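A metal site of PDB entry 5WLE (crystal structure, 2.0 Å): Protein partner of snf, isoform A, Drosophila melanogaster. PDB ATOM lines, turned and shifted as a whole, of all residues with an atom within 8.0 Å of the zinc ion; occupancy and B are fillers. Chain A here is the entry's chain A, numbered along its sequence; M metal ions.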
ATOM      1  N   TRP A  10      15.094  11.843 -13.448  1.00  0.00           N
ATOM      2  CA  TRP A  10      13.808  11.177 -13.584  1.00  0.00           C
ATOM      3  C   TRP A  10      13.189  11.431 -14.958  1.00  0.00           C
ATOM      4  O   TRP A  10      13.641  12.301 -15.715  1.00  0.00           O
ATOM      5  CB  TRP A  10      12.796  11.666 -12.530  1.00  0.00           C
ATOM      6  CG  TRP A  10      13.049  11.253 -11.118  1.00  0.00           C
ATOM      7  CD1 TRP A  10      13.483  12.036 -10.096  1.00  0.00           C
ATOM      8  CD2 TRP A  10      12.807   9.953 -10.561  1.00  0.00           C
ATOM      9  NE1 TRP A  10      13.549  11.305  -8.932  1.00  0.00           N
ATOM     10  CE2 TRP A  10      13.138  10.019  -9.196  1.00  0.00           C
ATOM     11  CE3 TRP A  10      12.351   8.738 -11.091  1.00  0.00           C
ATOM     12  CZ2 TRP A  10      13.021   8.913  -8.346  1.00  0.00           C
ATOM     13  CZ3 TRP A  10      12.243   7.643 -10.244  1.00  0.00           C
ATOM     14  CH2 TRP A  10      12.570   7.728  -8.890  1.00  0.00           C
ATOM     15  N   CYS A  11      12.143  10.663 -15.286  1.00  0.00           N
ATOM     16  CA  CYS A  11      11.133  11.072 -16.254  1.00  0.00           C
ATOM     17  C   CYS A  11      11.638  10.962 -17.705  1.00  0.00           C
ATOM     18  O   CYS A  11      12.787  10.566 -17.945  1.00  0.00           O
ATOM     19  CB  CYS A  11      10.665  12.505 -15.920  1.00  0.00           C
ATOM     20  SG  CYS A  11       9.277  13.204 -16.899  1.00  0.00           S
ATOM     21  N   ILE A  12      10.763  11.277 -18.654  1.00  0.00           N
ATOM     22  CA  ILE A  12      11.165  11.372 -20.059  1.00  0.00           C
ATOM     23  C   ILE A  12      12.282  12.386 -20.220  1.00  0.00           C
ATOM     24  O   ILE A  12      13.226  12.179 -20.989  1.00  0.00           O
ATOM     25  CB  ILE A  12       9.952  11.737 -20.927  1.00  0.00           C
ATOM     26  CG1 ILE A  12       8.890  10.642 -20.848  1.00  0.00           C
ATOM     27  CG2 ILE A  12      10.369  12.001 -22.385  1.00  0.00           C
ATOM     28  CD1 ILE A  12       7.497  11.106 -21.299  1.00  0.00           C
ATOM     29  N   CYS A  13      12.216  13.501 -19.469  1.00  0.00           N
ATOM     30  CA  CYS A  13      13.099  14.645 -19.667  1.00  0.00           C
ATOM     31  C   CYS A  13      14.492  14.469 -19.055  1.00  0.00           C
ATOM     32  O   CYS A  13      15.369  15.290 -19.348  1.00  0.00           O
ATOM     33  CB  CYS A  13      12.445  15.908 -19.098  1.00  0.00           C
ATOM     34  SG  CYS A  13      12.189  15.866 -17.305  1.00  0.00           S
ATOM     35  N   ARG A  14      14.709  13.439 -18.239  1.00  0.00           N
ATOM     36  CA  ARG A  14      15.996  13.184 -17.580  1.00  0.00           C
ATOM     37  C   ARG A  14      16.454  14.396 -16.755  1.00  0.00           C
ATOM     38  O   ARG A  14      17.550  14.939 -16.950  1.00  0.00           O
ATOM     39  CB  ARG A  14      17.076  12.777 -18.604  1.00  0.00           C
ATOM     40  CG  ARG A  14      16.650  11.711 -19.625  1.00  0.00           C
ATOM     41  CD  ARG A  14      16.000  10.517 -18.951  1.00  0.00           C
ATOM     42  NE  ARG A  14      16.899   9.882 -17.989  1.00  0.00           N
ATOM     43  CZ  ARG A  14      16.485   9.240 -16.897  1.00  0.00           C
ATOM     44  NH1 ARG A  14      15.182   9.156 -16.637  1.00  0.00           N
ATOM     45  NH2 ARG A  14      17.378   8.692 -16.087  1.00  0.00           N
ATOM     46  N   GLN A  15      15.611  14.812 -15.823  1.00  0.00           N
ATOM     47  CA  GLN A  15      15.857  15.963 -14.965  1.00  0.00           C
ATOM     48  C   GLN A  15      15.497  15.603 -13.527  1.00  0.00           C
ATOM     49  O   GLN A  15      14.755  14.650 -13.293  1.00  0.00           O
ATOM     50  CB  GLN A  15      15.017  17.170 -15.400  1.00  0.00           C
ATOM     51  CG  GLN A  15      15.476  17.839 -16.686  1.00  0.00           C
ATOM     52  CD  GLN A  15      14.605  19.022 -17.022  1.00  0.00           C
ATOM     53  OE1 GLN A  15      14.080  19.683 -16.121  1.00  0.00           O
ATOM     54  NE2 GLN A  15      14.438  19.305 -18.311  1.00  0.00           N
ATOM     55  N   PRO A  16      15.998  16.360 -12.544  1.00  0.00           N
ATOM     56  CA  PRO A  16      15.655  16.080 -11.138  1.00  0.00           C
ATOM     57  C   PRO A  16      14.196  16.404 -10.847  1.00  0.00           C
ATOM     58  O   PRO A  16      13.462  16.971 -11.666  1.00  0.00           O
ATOM     59  CB  PRO A  16      16.598  16.992 -10.340  1.00  0.00           C
ATOM     60  CG  PRO A  16      17.665  17.416 -11.323  1.00  0.00           C
ATOM     61  CD  PRO A  16      16.972  17.452 -12.660  1.00  0.00           C
ATOM     62  N   ARG A  20       8.844  19.666  -8.123  1.00  0.00           N
ATOM     63  CA  ARG A  20       7.727  19.795  -9.041  1.00  0.00           C
ATOM     64  C   ARG A  20       6.704  18.689  -8.804  1.00  0.00           C
ATOM     65  O   ARG A  20       7.014  17.647  -8.217  1.00  0.00           O
ATOM     66  CB  ARG A  20       8.219  19.725 -10.484  1.00  0.00           C
ATOM     67  CG  ARG A  20       9.209  20.835 -10.849  1.00  0.00           C
ATOM     68  CD  ARG A  20       9.969  20.508 -12.134  1.00  0.00           C
ATOM     69  NE  ARG A  20       9.055  20.287 -13.250  1.00  0.00           N
ATOM     70  CZ  ARG A  20       9.435  19.971 -14.493  1.00  0.00           C
ATOM     71  NH1 ARG A  20      10.724  19.829 -14.776  1.00  0.00           N
ATOM     72  NH2 ARG A  20       8.517  19.786 -15.439  1.00  0.00           N
ATOM     73  N   PHE A  21       5.473  18.927  -9.277  1.00  0.00           N
ATOM     74  CA  PHE A  21       4.461  17.875  -9.231  1.00  0.00           C
ATOM     75  C   PHE A  21       4.888  16.682 -10.065  1.00  0.00           C
ATOM     76  O   PHE A  21       5.276  16.829 -11.229  1.00  0.00           O
ATOM     77  CB  PHE A  21       3.107  18.379  -9.734  1.00  0.00           C
ATOM     78  CG  PHE A  21       2.139  17.267 -10.046  1.00  0.00           C
ATOM     79  CD1 PHE A  21       1.688  16.410  -9.046  1.00  0.00           C
ATOM     80  CD2 PHE A  21       1.711  17.044 -11.356  1.00  0.00           C
ATOM     81  CE1 PHE A  21       0.801  15.362  -9.327  1.00  0.00           C
ATOM     82  CE2 PHE A  21       0.821  16.004 -11.649  1.00  0.00           C
ATOM     83  CZ  PHE A  21       0.382  15.160 -10.632  1.00  0.00           C
ATOM     84  N   MET A  22       4.837  15.490  -9.461  1.00  0.00           N
ATOM     85  CA  MET A  22       5.209  14.273 -10.161  1.00  0.00           C
ATOM     86  C   MET A  22       4.184  13.193  -9.865  1.00  0.00           C
ATOM     87  O   MET A  22       3.512  13.204  -8.824  1.00  0.00           O
ATOM     88  CB  MET A  22       6.613  13.795  -9.761  1.00  0.00           C
ATOM     89  CG  MET A  22       7.715  14.824 -10.054  1.00  0.00           C
ATOM     90  SD  MET A  22       9.390  14.167  -9.955  1.00  0.00           S
ATOM     91  CE  MET A  22       9.503  13.237 -11.481  1.00  0.00           C
ATOM     92  N   TRP A  31       8.876   7.787 -11.580  1.00  0.00           N
ATOM     93  CA  TRP A  31       8.204   9.062 -11.388  1.00  0.00           C
ATOM     94  C   TRP A  31       8.376   9.968 -12.602  1.00  0.00           C
ATOM     95  O   TRP A  31       9.457  10.015 -13.208  1.00  0.00           O
ATOM     96  CB  TRP A  31       8.727   9.766 -10.138  1.00  0.00           C
ATOM     97  CG  TRP A  31       8.335   9.103  -8.874  1.00  0.00           C
ATOM     98  CD1 TRP A  31       9.021   8.123  -8.204  1.00  0.00           C
ATOM     99  CD2 TRP A  31       7.161   9.385  -8.096  1.00  0.00           C
ATOM    100  NE1 TRP A  31       8.331   7.767  -7.067  1.00  0.00           N
ATOM    101  CE2 TRP A  31       7.203   8.537  -6.965  1.00  0.00           C
ATOM    102  CE3 TRP A  31       6.091  10.271  -8.230  1.00  0.00           C
ATOM    103  CZ2 TRP A  31       6.203   8.544  -5.991  1.00  0.00           C
ATOM    104  CZ3 TRP A  31       5.091  10.278  -7.257  1.00  0.00           C
ATOM    105  CH2 TRP A  31       5.160   9.420  -6.150  1.00  0.00           C
ATOM    106  N   PHE A  32       7.327  10.717 -12.919  1.00  0.00           N
ATOM    107  CA  PHE A  32       7.276  11.570 -14.099  1.00  0.00           C
ATOM    108  C   PHE A  32       6.744  12.931 -13.706  1.00  0.00           C
ATOM    109  O   PHE A  32       5.791  13.036 -12.934  1.00  0.00           O
ATOM    110  CB  PHE A  32       6.390  10.921 -15.182  1.00  0.00           C
ATOM    111  CG  PHE A  32       6.920   9.611 -15.673  1.00  0.00           C
ATOM    112  CD1 PHE A  32       6.726   8.444 -14.946  1.00  0.00           C
ATOM    113  CD2 PHE A  32       7.665   9.546 -16.843  1.00  0.00           C
ATOM    114  CE1 PHE A  32       7.247   7.240 -15.376  1.00  0.00           C
ATOM    115  CE2 PHE A  32       8.182   8.360 -17.284  1.00  0.00           C
ATOM    116  CZ  PHE A  32       7.970   7.193 -16.544  1.00  0.00           C
ATOM    117  N   HIS A  33       7.398  13.991 -14.202  1.00  0.00           N
ATOM    118  CA  HIS A  33       6.840  15.328 -14.026  1.00  0.00           C
ATOM    119  C   HIS A  33       5.503  15.381 -14.735  1.00  0.00           C
ATOM    120  O   HIS A  33       5.372  14.934 -15.876  1.00  0.00           O
ATOM    121  CB  HIS A  33       7.766  16.403 -14.590  1.00  0.00           C
ATOM    122  CG  HIS A  33       9.170  16.339 -14.085  1.00  0.00           C
ATOM    123  ND1 HIS A  33      10.229  15.903 -14.846  1.00  0.00           N
ATOM    124  CD2 HIS A  33       9.708  16.686 -12.888  1.00  0.00           C
ATOM    125  CE1 HIS A  33      11.347  15.966 -14.154  1.00  0.00           C
ATOM    126  NE2 HIS A  33      11.057  16.441 -12.955  1.00  0.00           N
ATOM    127  N   GLY A  34       4.484  15.884 -14.049  1.00  0.00           N
ATOM    128  CA  GLY A  34       3.203  16.090 -14.704  1.00  0.00           C
ATOM    129  C   GLY A  34       3.302  16.836 -16.020  1.00  0.00           C
ATOM    130  O   GLY A  34       2.608  16.513 -16.989  1.00  0.00           O
ATOM    131  N   THR A  35       4.172  17.861 -16.069  1.00  0.00           N
ATOM    132  CA  THR A  35       4.355  18.635 -17.301  1.00  0.00           C
ATOM    133  C   THR A  35       4.650  17.728 -18.482  1.00  0.00           C
ATOM    134  O   THR A  35       4.090  17.905 -19.571  1.00  0.00           O
ATOM    135  CB  THR A  35       5.504  19.649 -17.171  1.00  0.00           C
ATOM    136  OG1 THR A  35       5.438  20.337 -15.912  1.00  0.00           O
ATOM    137  CG2 THR A  35       5.416  20.675 -18.294  1.00  0.00           C
ATOM    138  N   CYS A  36       5.544  16.768 -18.288  1.00  0.00           N
ATOM    139  CA  CYS A  36       6.095  15.998 -19.395  1.00  0.00           C
ATOM    140  C   CYS A  36       5.154  14.914 -19.879  1.00  0.00           C
ATOM    141  O   CYS A  36       5.317  14.422 -21.003  1.00  0.00           O
ATOM    142  CB  CYS A  36       7.419  15.373 -18.956  1.00  0.00           C
ATOM    143  SG  CYS A  36       8.586  16.588 -18.331  1.00  0.00           S
ATOM    144  N   VAL A  37       4.189  14.507 -19.057  1.00  0.00           N
ATOM    145  CA  VAL A  37       3.215  13.508 -19.453  1.00  0.00           C
ATOM    146  C   VAL A  37       1.825  14.104 -19.592  1.00  0.00           C
ATOM    147  O   VAL A  37       0.854  13.368 -19.773  1.00  0.00           O
ATOM    148  CB  VAL A  37       3.213  12.328 -18.460  1.00  0.00           C
ATOM    149  CG1 VAL A  37       4.553  11.604 -18.553  1.00  0.00           C
ATOM    150  CG2 VAL A  37       2.943  12.806 -17.031  1.00  0.00           C
HETATM  151 ZN    ZN M   1      10.021  15.397 -16.958  1.00  0.00          ZN
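NH1 of Arg 14 is in hydrogen-bond range of O of Cys 11 (3.1 Å). NE2 of His 33 is in hydrogen-bond range of O of Pro 16 (2.8 Å). N of Cys 11 is in hydrogen-bond range of O of Trp 31, 3.5 Å away.
ND1 of His 33 is bound to the zinc ion (2.2 Å). The zinc ion is bound by the side-chain sulfur (SG) of Cys 13. SG of Cys 36 binds the zinc ion (2.3 Å). The zinc ion is bound by SG of Cys 11, 2.3 Å away.
The nearest printed residue that does not touch the zinc ion is Ile 12 (4.5 Å).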
